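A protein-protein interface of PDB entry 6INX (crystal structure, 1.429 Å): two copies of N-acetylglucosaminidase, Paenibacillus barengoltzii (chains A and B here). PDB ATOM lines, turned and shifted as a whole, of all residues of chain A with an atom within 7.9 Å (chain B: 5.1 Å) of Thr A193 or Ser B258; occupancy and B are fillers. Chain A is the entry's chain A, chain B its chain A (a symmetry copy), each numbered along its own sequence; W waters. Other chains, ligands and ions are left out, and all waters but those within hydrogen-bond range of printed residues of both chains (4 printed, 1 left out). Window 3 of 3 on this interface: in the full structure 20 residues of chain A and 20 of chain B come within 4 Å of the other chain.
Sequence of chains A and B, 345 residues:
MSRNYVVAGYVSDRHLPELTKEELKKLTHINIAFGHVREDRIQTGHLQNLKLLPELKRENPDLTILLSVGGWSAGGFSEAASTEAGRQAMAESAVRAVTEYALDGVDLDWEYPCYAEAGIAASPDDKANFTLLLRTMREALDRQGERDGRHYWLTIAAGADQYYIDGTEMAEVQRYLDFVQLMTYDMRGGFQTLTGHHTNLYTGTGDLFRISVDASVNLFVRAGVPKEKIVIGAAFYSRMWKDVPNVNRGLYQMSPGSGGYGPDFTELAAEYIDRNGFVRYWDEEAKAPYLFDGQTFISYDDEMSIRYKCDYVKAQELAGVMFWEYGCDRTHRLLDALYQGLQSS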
ATOM      1  N   GLY A 189     -26.880  12.237 -16.927  1.00  0.00           N
ATOM      2  CA  GLY A 189     -27.948  11.288 -17.160  1.00  0.00           C
ATOM      3  C   GLY A 189     -29.189  11.938 -17.732  1.00  0.00           C
ATOM      4  O   GLY A 189     -29.125  12.573 -18.786  1.00  0.00           O
ATOM      5  N   GLY A 190     -30.310  11.834 -17.019  1.00  0.00           N
ATOM      6  CA  GLY A 190     -31.603  12.160 -17.603  1.00  0.00           C
ATOM      7  C   GLY A 190     -31.881  13.640 -17.793  1.00  0.00           C
ATOM      8  O   GLY A 190     -32.904  13.981 -18.401  1.00  0.00           O
ATOM      9  N   PHE A 191     -31.017  14.522 -17.301  1.00  0.00           N
ATOM     10  CA  PHE A 191     -31.231  15.955 -17.468  1.00  0.00           C
ATOM     11  C   PHE A 191     -30.331  16.594 -18.519  1.00  0.00           C
ATOM     12  O   PHE A 191     -30.446  17.801 -18.755  1.00  0.00           O
ATOM     13  CB  PHE A 191     -31.057  16.686 -16.133  1.00  0.00           C
ATOM     14  CG  PHE A 191     -32.072  16.287 -15.098  1.00  0.00           C
ATOM     15  CD1 PHE A 191     -33.399  16.616 -15.267  1.00  0.00           C
ATOM     16  CD2 PHE A 191     -31.701  15.552 -13.982  1.00  0.00           C
ATOM     17  CE1 PHE A 191     -34.352  16.245 -14.323  1.00  0.00           C
ATOM     18  CE2 PHE A 191     -32.652  15.178 -13.041  1.00  0.00           C
ATOM     19  CZ  PHE A 191     -33.974  15.528 -13.218  1.00  0.00           C
ATOM     20  N   GLN A 192     -29.454  15.833 -19.174  1.00  0.00           N
ATOM     21  CA  GLN A 192     -28.567  16.430 -20.163  1.00  0.00           C
ATOM     22  C   GLN A 192     -28.542  15.615 -21.449  1.00  0.00           C
ATOM     23  O   GLN A 192     -28.604  14.383 -21.432  1.00  0.00           O
ATOM     24  CB  GLN A 192     -27.144  16.660 -19.604  1.00  0.00           C
ATOM     25  CG  GLN A 192     -26.380  15.392 -19.288  1.00  0.00           C
ATOM     26  CD  GLN A 192     -25.021  15.701 -18.702  1.00  0.00           C
ATOM     27  OE1 GLN A 192     -24.915  16.141 -17.553  1.00  0.00           O
ATOM     28  NE2 GLN A 192     -23.968  15.503 -19.506  1.00  0.00           N
ATOM     29  N   THR A 193     -28.419  16.335 -22.566  1.00  0.00           N
ATOM     30  CA  THR A 193     -28.314  15.717 -23.878  1.00  0.00           C
ATOM     31  C   THR A 193     -26.873  15.605 -24.351  1.00  0.00           C
ATOM     32  O   THR A 193     -26.630  15.050 -25.427  1.00  0.00           O
ATOM     33  CB  THR A 193     -29.117  16.509 -24.912  1.00  0.00           C
ATOM     34  OG1 THR A 193     -28.661  17.864 -24.911  1.00  0.00           O
ATOM     35  CG2 THR A 193     -30.604  16.486 -24.594  1.00  0.00           C
ATOM     36  N   LEU A 194     -25.912  16.095 -23.570  1.00  0.00           N
ATOM     37  CA  LEU A 194     -24.500  15.922 -23.895  1.00  0.00           C
ATOM     38  C   LEU A 194     -24.008  14.613 -23.291  1.00  0.00           C
ATOM     39  O   LEU A 194     -24.248  14.345 -22.111  1.00  0.00           O
ATOM     40  CB  LEU A 194     -23.688  17.071 -23.299  1.00  0.00           C
ATOM     41  CG  LEU A 194     -22.255  17.096 -23.824  1.00  0.00           C
ATOM     42  CD1 LEU A 194     -22.231  17.541 -25.276  1.00  0.00           C
ATOM     43  CD2 LEU A 194     -21.402  18.031 -22.970  1.00  0.00           C
ATOM     44  N   THR A 195     -23.317  13.803 -24.092  1.00  0.00           N
ATOM     45  CA  THR A 195     -22.785  12.564 -23.555  1.00  0.00           C
ATOM     46  C   THR A 195     -21.618  12.841 -22.612  1.00  0.00           C
ATOM     47  O   THR A 195     -20.944  13.880 -22.677  1.00  0.00           O
ATOM     48  CB  THR A 195     -22.312  11.624 -24.666  1.00  0.00           C
ATOM     49  OG1 THR A 195     -21.182  12.194 -25.347  1.00  0.00           O
ATOM     50  CG2 THR A 195     -23.416  11.363 -25.678  1.00  0.00           C
ATOM     51  N   GLY A 196     -21.396  11.893 -21.715  1.00  0.00           N
ATOM     52  CA  GLY A 196     -20.259  11.957 -20.821  1.00  0.00           C
ATOM     53  C   GLY A 196     -20.318  10.796 -19.850  1.00  0.00           C
ATOM     54  O   GLY A 196     -21.180   9.928 -19.951  1.00  0.00           O
ATOM     55  N   PHE A 209     -19.652  19.800 -18.524  1.00  0.00           N
ATOM     56  CA  PHE A 209     -20.070  19.471 -17.171  1.00  0.00           C
ATOM     57  C   PHE A 209     -18.834  19.028 -16.402  1.00  0.00           C
ATOM     58  O   PHE A 209     -18.021  18.262 -16.928  1.00  0.00           O
ATOM     59  CB  PHE A 209     -21.128  18.370 -17.226  1.00  0.00           C
ATOM     60  CG  PHE A 209     -22.389  18.802 -17.921  1.00  0.00           C
ATOM     61  CD1 PHE A 209     -23.430  19.364 -17.194  1.00  0.00           C
ATOM     62  CD2 PHE A 209     -22.528  18.676 -19.286  1.00  0.00           C
ATOM     63  CE1 PHE A 209     -24.588  19.786 -17.832  1.00  0.00           C
ATOM     64  CE2 PHE A 209     -23.688  19.101 -19.933  1.00  0.00           C
ATOM     65  CZ  PHE A 209     -24.717  19.646 -19.194  1.00  0.00           C
ATOM     66  N   TRP A 241     -26.838   7.302 -24.235  1.00  0.00           N
ATOM     67  CA  TRP A 241     -27.402   8.305 -25.124  1.00  0.00           C
ATOM     68  C   TRP A 241     -27.511   7.729 -26.532  1.00  0.00           C
ATOM     69  O   TRP A 241     -26.632   6.981 -26.981  1.00  0.00           O
ATOM     70  CB  TRP A 241     -26.512   9.554 -25.184  1.00  0.00           C
ATOM     71  CG  TRP A 241     -26.515  10.430 -23.960  1.00  0.00           C
ATOM     72  CD1 TRP A 241     -27.178  11.613 -23.808  1.00  0.00           C
ATOM     73  CD2 TRP A 241     -25.794  10.210 -22.742  1.00  0.00           C
ATOM     74  NE1 TRP A 241     -26.914  12.152 -22.565  1.00  0.00           N
ATOM     75  CE2 TRP A 241     -26.063  11.312 -21.893  1.00  0.00           C
ATOM     76  CE3 TRP A 241     -24.950   9.190 -22.283  1.00  0.00           C
ATOM     77  CZ2 TRP A 241     -25.527  11.413 -20.609  1.00  0.00           C
ATOM     78  CZ3 TRP A 241     -24.403   9.300 -21.016  1.00  0.00           C
ATOM     79  CH2 TRP A 241     -24.699  10.403 -20.188  1.00  0.00           C
ATOM     80  N   LYS A 242     -28.569   8.118 -27.241  1.00  0.00           N
ATOM     81  CA  LYS A 242     -28.867   7.571 -28.554  1.00  0.00           C
ATOM     82  C   LYS A 242     -28.670   8.606 -29.655  1.00  0.00           C
ATOM     83  O   LYS A 242     -28.804   9.812 -29.433  1.00  0.00           O
ATOM     84  CB  LYS A 242     -30.307   7.066 -28.601  1.00  0.00           C
ATOM     85  CG  LYS A 242     -30.604   5.988 -27.556  1.00  0.00           C
ATOM     86  CD  LYS A 242     -32.072   5.592 -27.590  1.00  0.00           C
ATOM     87  CE  LYS A 242     -32.354   4.496 -26.568  1.00  0.00           C
ATOM     88  NZ  LYS A 242     -33.793   4.099 -26.537  1.00  0.00           N
ATOM     89  N   ASP A 243     -28.347   8.105 -30.851  1.00  0.00           N
ATOM     90  CA  ASP A 243     -28.300   8.924 -32.062  1.00  0.00           C
ATOM     91  C   ASP A 243     -27.307  10.076 -31.931  1.00  0.00           C
ATOM     92  O   ASP A 243     -27.614  11.236 -32.217  1.00  0.00           O
ATOM     93  CB  ASP A 243     -29.700   9.392 -32.450  1.00  0.00           C
ATOM     94  CG  ASP A 243     -30.642   8.227 -32.675  1.00  0.00           C
ATOM     95  OD1 ASP A 243     -30.266   7.309 -33.437  1.00  0.00           O
ATOM     96  OD2 ASP A 243     -31.728   8.221 -32.069  1.00  0.00           O
ATOM     97  N   VAL A 244     -26.096   9.738 -31.507  1.00  0.00           N
ATOM     98  CA  VAL A 244     -25.072  10.761 -31.312  1.00  0.00           C
ATOM     99  C   VAL A 244     -24.109  10.761 -32.493  1.00  0.00           C
ATOM    100  O   VAL A 244     -23.835   9.700 -33.076  1.00  0.00           O
ATOM    101  CB  VAL A 244     -24.351  10.622 -29.962  1.00  0.00           C
ATOM    102  CG1 VAL A 244     -25.340  10.334 -28.844  1.00  0.00           C
ATOM    103  CG2 VAL A 244     -23.331   9.558 -30.017  1.00  0.00           C
ATOM    104  N   PRO A 245     -23.615  11.927 -32.900  1.00  0.00           N
ATOM    105  CA  PRO A 245     -22.689  11.990 -34.034  1.00  0.00           C
ATOM    106  C   PRO A 245     -21.445  11.144 -33.805  1.00  0.00           C
ATOM    107  O   PRO A 245     -20.921  11.048 -32.691  1.00  0.00           O
ATOM    108  CB  PRO A 245     -22.331  13.481 -34.105  1.00  0.00           C
ATOM    109  CG  PRO A 245     -23.497  14.168 -33.485  1.00  0.00           C
ATOM    110  CD  PRO A 245     -24.005  13.259 -32.413  1.00  0.00           C
ATOM    111  N   TYR A 252     -18.772  13.567 -25.415  1.00  0.00           N
ATOM    112  CA  TYR A 252     -19.037  15.013 -25.426  1.00  0.00           C
ATOM    113  C   TYR A 252     -19.721  15.444 -26.720  1.00  0.00           C
ATOM    114  O   TYR A 252     -19.416  16.491 -27.295  1.00  0.00           O
ATOM    115  CB  TYR A 252     -17.802  15.865 -25.080  1.00  0.00           C
ATOM    116  CG  TYR A 252     -17.093  15.351 -23.854  1.00  0.00           C
ATOM    117  CD1 TYR A 252     -17.818  14.875 -22.769  1.00  0.00           C
ATOM    118  CD2 TYR A 252     -15.714  15.291 -23.794  1.00  0.00           C
ATOM    119  CE1 TYR A 252     -17.191  14.383 -21.653  1.00  0.00           C
ATOM    120  CE2 TYR A 252     -15.077  14.792 -22.671  1.00  0.00           C
ATOM    121  CZ  TYR A 252     -15.830  14.333 -21.610  1.00  0.00           C
ATOM    122  OH  TYR A 252     -15.223  13.815 -20.484  1.00  0.00           O
ATOM    123  N   GLN A 253     -20.658  14.617 -27.179  1.00  0.00           N
ATOM    124  CA  GLN A 253     -21.471  14.858 -28.357  1.00  0.00           C
ATOM    125  C   GLN A 253     -22.920  15.067 -27.943  1.00  0.00           C
ATOM    126  O   GLN A 253     -23.365  14.604 -26.887  1.00  0.00           O
ATOM    127  CB  GLN A 253     -21.406  13.661 -29.309  1.00  0.00           C
ATOM    128  CG  GLN A 253     -20.003  13.309 -29.771  1.00  0.00           C
ATOM    129  CD  GLN A 253     -19.311  14.472 -30.435  1.00  0.00           C
ATOM    130  OE1 GLN A 253     -19.834  15.064 -31.380  1.00  0.00           O
ATOM    131  NE2 GLN A 253     -18.135  14.828 -29.925  1.00  0.00           N
ATOM    132  N   MET A 254     -23.671  15.739 -28.809  1.00  0.00           N
ATOM    133  CA  MET A 254     -25.053  16.073 -28.500  1.00  0.00           C
ATOM    134  C   MET A 254     -25.985  15.011 -29.071  1.00  0.00           C
ATOM    135  O   MET A 254     -25.920  14.684 -30.261  1.00  0.00           O
ATOM    136  CB  MET A 254     -25.428  17.446 -29.061  1.00  0.00           C
ATOM    137  CG  MET A 254     -26.771  17.964 -28.520  1.00  0.00           C
ATOM    138  SD  MET A 254     -27.404  19.388 -29.418  1.00  0.00           S
ATOM    139  CE  MET A 254     -26.595  20.709 -28.535  1.00  0.00           C
ATOM    140  N   SER A 255     -26.854  14.476 -28.212  1.00  0.00           N
ATOM    141  CA  SER A 255     -27.940  13.580 -28.555  1.00  0.00           C
ATOM    142  C   SER A 255     -29.241  14.368 -28.657  1.00  0.00           C
ATOM    143  O   SER A 255     -29.386  15.419 -28.025  1.00  0.00           O
ATOM    144  CB  SER A 255     -28.100  12.543 -27.437  1.00  0.00           C
ATOM    145  OG  SER A 255     -29.211  11.696 -27.680  1.00  0.00           O
ATOM    146  N   PRO A 256     -30.214  13.894 -29.439  1.00  0.00           N
ATOM    147  CA  PRO A 256     -31.555  14.503 -29.389  1.00  0.00           C
ATOM    148  C   PRO A 256     -32.258  14.309 -28.056  1.00  0.00           C
ATOM    149  O   PRO A 256     -33.184  15.065 -27.742  1.00  0.00           O
ATOM    150  CB  PRO A 256     -32.319  13.782 -30.512  1.00  0.00           C
ATOM    151  CG  PRO A 256     -31.274  13.158 -31.365  1.00  0.00           C
ATOM    152  CD  PRO A 256     -30.115  12.841 -30.466  1.00  0.00           C
ATOM    153  N   GLY A 257     -31.853  13.311 -27.269  1.00  0.00           N
ATOM    154  CA  GLY A 257     -32.496  13.015 -26.008  1.00  0.00           C
ATOM    155  C   GLY A 257     -31.473  12.945 -24.886  1.00  0.00           C
ATOM    156  O   GLY A 257     -30.267  13.024 -25.115  1.00  0.00           O
ATOM    157  N   SER A 258     -31.991  12.749 -23.678  1.00  0.00           N
ATOM    158  CA  SER A 258     -31.119  12.723 -22.511  1.00  0.00           C
ATOM    159  C   SER A 258     -30.502  11.335 -22.329  1.00  0.00           C
ATOM    160  O   SER A 258     -30.744  10.403 -23.100  1.00  0.00           O
ATOM    161  CB  SER A 258     -31.888  13.158 -21.271  1.00  0.00           C
ATOM    162  OG  SER A 258     -32.946  12.263 -21.011  1.00  0.00           O
ATOM    163  N   GLY A 259     -29.659  11.206 -21.307  1.00  0.00           N
ATOM    164  CA  GLY A 259     -29.001   9.951 -21.014  1.00  0.00           C
ATOM    165  C   GLY A 259     -29.847   9.089 -20.104  1.00  0.00           C
ATOM    166  O   GLY A 259     -29.802   9.225 -18.883  1.00  0.00           O
ATOM    167  N   GLY B 189     -30.004  25.600 -22.024  1.00  0.00           N
ATOM    168  CA  GLY B 189     -30.416  25.584 -23.411  1.00  0.00           C
ATOM    169  C   GLY B 189     -30.275  24.217 -24.044  1.00  0.00           C
ATOM    170  O   GLY B 189     -30.855  23.246 -23.556  1.00  0.00           O
ATOM    171  N   GLY B 190     -29.465  24.120 -25.098  1.00  0.00           N
ATOM    172  CA  GLY B 190     -29.482  22.939 -25.950  1.00  0.00           C
ATOM    173  C   GLY B 190     -28.840  21.696 -25.361  1.00  0.00           C
ATOM    174  O   GLY B 190     -28.935  20.627 -25.977  1.00  0.00           O
ATOM    175  N   PHE B 191     -28.198  21.797 -24.202  1.00  0.00           N
ATOM    176  CA  PHE B 191     -27.575  20.630 -23.586  1.00  0.00           C
ATOM    177  C   PHE B 191     -28.348  20.074 -22.398  1.00  0.00           C
ATOM    178  O   PHE B 191     -27.919  19.071 -21.818  1.00  0.00           O
ATOM    179  CB  PHE B 191     -26.138  20.948 -23.158  1.00  0.00           C
ATOM    180  CG  PHE B 191     -25.231  21.278 -24.311  1.00  0.00           C
ATOM    181  CD1 PHE B 191     -24.892  20.304 -25.225  1.00  0.00           C
ATOM    182  CD2 PHE B 191     -24.753  22.566 -24.496  1.00  0.00           C
ATOM    183  CE1 PHE B 191     -24.062  20.595 -26.303  1.00  0.00           C
ATOM    184  CE2 PHE B 191     -23.926  22.859 -25.574  1.00  0.00           C
ATOM    185  CZ  PHE B 191     -23.586  21.869 -26.472  1.00  0.00           C
ATOM    186  N   GLN B 192     -29.482  20.667 -22.024  1.00  0.00           N
ATOM    187  CA  GLN B 192     -30.222  20.165 -20.874  1.00  0.00           C
ATOM    188  C   GLN B 192     -31.706  20.030 -21.187  1.00  0.00           C
ATOM    189  O   GLN B 192     -32.289  20.842 -21.910  1.00  0.00           O
ATOM    190  CB  GLN B 192     -29.980  21.021 -19.609  1.00  0.00           C
ATOM    191  CG  GLN B 192     -30.528  22.430 -19.688  1.00  0.00           C
ATOM    192  CD  GLN B 192     -30.209  23.214 -18.436  1.00  0.00           C
ATOM    193  OE1 GLN B 192     -29.056  23.594 -18.206  1.00  0.00           O
ATOM    194  NE2 GLN B 192     -31.229  23.434 -17.595  1.00  0.00           N
ATOM    195  N   THR B 193     -32.311  18.996 -20.597  1.00  0.00           N
ATOM    196  CA  THR B 193     -33.738  18.753 -20.733  1.00  0.00           C
ATOM    197  C   THR B 193     -34.531  19.287 -19.551  1.00  0.00           C
ATOM    198  O   THR B 193     -35.762  19.198 -19.558  1.00  0.00           O
ATOM    199  CB  THR B 193     -34.016  17.256 -20.884  1.00  0.00           C
ATOM    200  OG1 THR B 193     -33.451  16.567 -19.767  1.00  0.00           O
ATOM    201  CG2 THR B 193     -33.408  16.706 -22.165  1.00  0.00           C
ATOM    202  N   MET B 240     -36.551  27.661 -25.184  1.00  0.00           N
ATOM    203  CA  MET B 240     -37.876  27.063 -25.078  1.00  0.00           C
ATOM    204  C   MET B 240     -37.782  25.551 -24.965  1.00  0.00           C
ATOM    205  O   MET B 240     -37.008  24.915 -25.681  1.00  0.00           O
ATOM    206  CB  MET B 240     -38.700  27.427 -26.320  1.00  0.00           C
ATOM    207  CG  MET B 240     -40.083  26.801 -26.368  1.00  0.00           C
ATOM    208  SD  MET B 240     -41.041  27.400 -27.789  1.00  0.00           S
ATOM    209  CE  MET B 240     -40.124  26.667 -29.133  1.00  0.00           C
ATOM    210  N   TRP B 241     -38.565  24.983 -24.048  1.00  0.00           N
ATOM    211  CA  TRP B 241     -38.675  23.542 -23.897  1.00  0.00           C
ATOM    212  C   TRP B 241     -40.110  23.111 -24.181  1.00  0.00           C
ATOM    213  O   TRP B 241     -41.066  23.809 -23.816  1.00  0.00           O
ATOM    214  CB  TRP B 241     -38.317  23.106 -22.470  1.00  0.00           C
ATOM    215  CG  TRP B 241     -36.859  23.178 -22.100  1.00  0.00           C
ATOM    216  CD1 TRP B 241     -35.987  22.131 -22.023  1.00  0.00           C
ATOM    217  CD2 TRP B 241     -36.123  24.347 -21.722  1.00  0.00           C
ATOM    218  NE1 TRP B 241     -34.745  22.573 -21.616  1.00  0.00           N
ATOM    219  CE2 TRP B 241     -34.804  23.930 -21.420  1.00  0.00           C
ATOM    220  CE3 TRP B 241     -36.447  25.706 -21.612  1.00  0.00           C
ATOM    221  CZ2 TRP B 241     -33.809  24.826 -21.027  1.00  0.00           C
ATOM    222  CZ3 TRP B 241     -35.466  26.592 -21.204  1.00  0.00           C
ATOM    223  CH2 TRP B 241     -34.157  26.150 -20.922  1.00  0.00           C
ATOM    224  N   SER B 255     -38.319  17.960 -19.819  1.00  0.00           N
ATOM    225  CA  SER B 255     -38.792  17.840 -21.183  1.00  0.00           C
ATOM    226  C   SER B 255     -38.176  16.606 -21.832  1.00  0.00           C
ATOM    227  O   SER B 255     -37.092  16.167 -21.435  1.00  0.00           O
ATOM    228  CB  SER B 255     -38.335  19.070 -21.977  1.00  0.00           C
ATOM    229  OG  SER B 255     -38.694  18.959 -23.344  1.00  0.00           O
ATOM    230  N   PRO B 256     -38.832  16.018 -22.835  1.00  0.00           N
ATOM    231  CA  PRO B 256     -38.169  14.967 -23.627  1.00  0.00           C
ATOM    232  C   PRO B 256     -36.986  15.474 -24.434  1.00  0.00           C
ATOM    233  O   PRO B 256     -36.128  14.674 -24.822  1.00  0.00           O
ATOM    234  CB  PRO B 256     -39.282  14.464 -24.562  1.00  0.00           C
ATOM    235  CG  PRO B 256     -40.553  14.941 -23.956  1.00  0.00           C
ATOM    236  CD  PRO B 256     -40.236  16.220 -23.238  1.00  0.00           C
ATOM    237  N   GLY B 257     -36.921  16.779 -24.706  1.00  0.00           N
ATOM    238  CA  GLY B 257     -35.861  17.345 -25.512  1.00  0.00           C
ATOM    239  C   GLY B 257     -35.203  18.511 -24.791  1.00  0.00           C
ATOM    240  O   GLY B 257     -35.642  18.932 -23.722  1.00  0.00           O
ATOM    241  N   SER B 258     -34.169  19.044 -25.434  1.00  0.00           N
ATOM    242  CA  SER B 258     -33.416  20.129 -24.820  1.00  0.00           C
ATOM    243  C   SER B 258     -34.099  21.473 -25.075  1.00  0.00           C
ATOM    244  O   SER B 258     -35.149  21.564 -25.718  1.00  0.00           O
ATOM    245  CB  SER B 258     -31.981  20.127 -25.331  1.00  0.00           C
ATOM    246  OG  SER B 258     -31.957  20.349 -26.724  1.00  0.00           O
ATOM    247  N   GLY B 259     -33.512  22.535 -24.529  1.00  0.00           N
ATOM    248  CA  GLY B 259     -34.047  23.870 -24.688  1.00  0.00           C
ATOM    249  C   GLY B 259     -33.513  24.528 -25.941  1.00  0.00           C
ATOM    250  O   GLY B 259     -32.437  25.122 -25.933  1.00  0.00           O
ATOM    251  N   GLY B 260     -34.251  24.394 -27.032  1.00  0.00           N
ATOM    252  CA  GLY B 260     -33.855  25.016 -28.271  1.00  0.00           C
ATOM    253  C   GLY B 260     -34.190  26.485 -28.269  1.00  0.00           C
ATOM    254  O   GLY B 260     -34.723  27.040 -27.311  1.00  0.00           O
HETATM  255  O   HOH W   1     -34.953  12.732 -23.488  1.00  0.00           O
HETATM  256  O   HOH W   2     -35.343  14.124 -20.752  1.00  0.00           O
HETATM  257  O   HOH W   3     -29.863  20.485 -28.463  1.00  0.00           O
HETATM  258  O   HOH W   4     -33.313  17.688 -27.932  1.00  0.00           O
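OG1 of Thr B193 sits at hydrogen-bond distance from O of Gly A190 (3.0 Å). The backbone carbonyl oxygen (O) of Phe A191 lies within hydrogen-bond range of the backbone NH (N) of Thr B193 (2.9 Å). OG1 of Thr A193 is in hydrogen-bond range of O of Gly B190. The backbone NH (N) of Thr A193 sits at hydrogen-bond distance from the backbone carbonyl oxygen (O) of Phe B191 (2.9 Å).
The backbone NH of Gly A190 sits at hydrogen-bond distance from the backbone carbonyl oxygen of Gly A259 (3.2 Å). The backbone carbonyl oxygen (O) of Leu A194 lies within hydrogen-bond range of the side-chain amide nitrogen (NE2) of Gln A192. The indole nitrogen of Trp A241 is in hydrogen-bond range of the backbone carbonyl oxygen of Gln A192, 3.0 Å away. OG of Ser B258 sits at hydrogen-bond distance from O of Gly B190 (3.1 Å). The backbone carbonyl oxygen (O) of Gly B259 lies within hydrogen-bond range of the backbone NH (N) of Gly B190, at 3.2 Å. O of Thr B193 is in hydrogen-bond range of N of Ser B255 (2.9 Å).
Among the printed residues, merely in contact across the chains: Phe A191 with Gln B192 (3.2 Å), Gln A192 with Phe B191 (3.2 Å), Met A254 with Phe B191 (3.4 Å), Met A254 with Gly B190 (3.5 Å), Leu A194 with Phe B191 (3.7 Å), Thr A193 with Thr B193 (3.7 Å), Thr A193 with Ser B258 (3.96 Å) and Ser A258 with Thr B193 (3.96 Å).
Of the printed residues of chain B, Gly A190 touches Thr B193. Printed residues of chain B within 4 Å of Gln A192: Phe B191. Of the printed residues of chain B, Met A254 touches Gly B190 and Phe B191. Printed residues of chain B within 4 Å of Ser A258: Thr B193. Of the printed residues of chain A, Thr B193 touches Gly A190 (3.0 Å), Phe A191 (2.9 Å), Thr A193 (3.7 Å) and Ser A258 (3.96 Å). No residue of chain A comes within 4 Å of Gly B257. Ser B258 touches just one residue of chain A: Thr A193 (3.96 Å). Gly B260 touches none of the printed residues of chain A. The nearest residue of chain B that does not touch Thr A193 is Gln B192 (4.1 Å). The nearest residue of chain A that does not touch Ser B258 is Pro A256 (4.7 Å).
Of the 13 printed residues of chain B, 5 touch a printed residue of chain A. Printed residues of chain B that touch a printed residue of chain A: Gly B190, Phe B191, Gln B192, Thr B193 and Ser B258. Hydrophobic or aromatic side chains of chain B that line the printed part of chain A: Phe B191. Of the 22 printed residues of chain A, 7 touch a printed residue of chain B.
Gly A190 touches Thr B193, and with the chains exchanged Thr A193 touches Gly B190. Phe A191 touches Gln B192, and with the chains exchanged Gln A192 touches Phe B191. Phe A191 touches Thr B193, and with the chains exchanged Thr A193 touches Phe B191. Thr A193 touches Ser B258, and with the chains exchanged Ser A258 touches Thr B193. 11 positions are printed for both chains. Of the 12 pairs that touch across the chains among the printed residues, 9 have their exchanged pair printed and touching as well.
Water W4 lies within hydrogen-bond range of O of Pro A256 (2.6 Å) and N of Ser B258 (3.0 Å). Water W1 bridges O of Pro B256 (2.6 Å) and N of Ser A258 (3.0 Å). Water W3 lies within hydrogen-bond range of the backbone carbonyl oxygen of Gly B190 (2.7 Å), the side-chain hydroxyl of Ser B258 (2.7 Å) and the side-chain sulfur of Met A254 (2.9 Å). Water W2 lies within hydrogen-bond range of the backbone carbonyl oxygen of Ser B255, the side-chain hydroxyl of Ser A258, the side-chain hydroxyl of Thr B193 and the backbone carbonyl oxygen of Gly A190.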
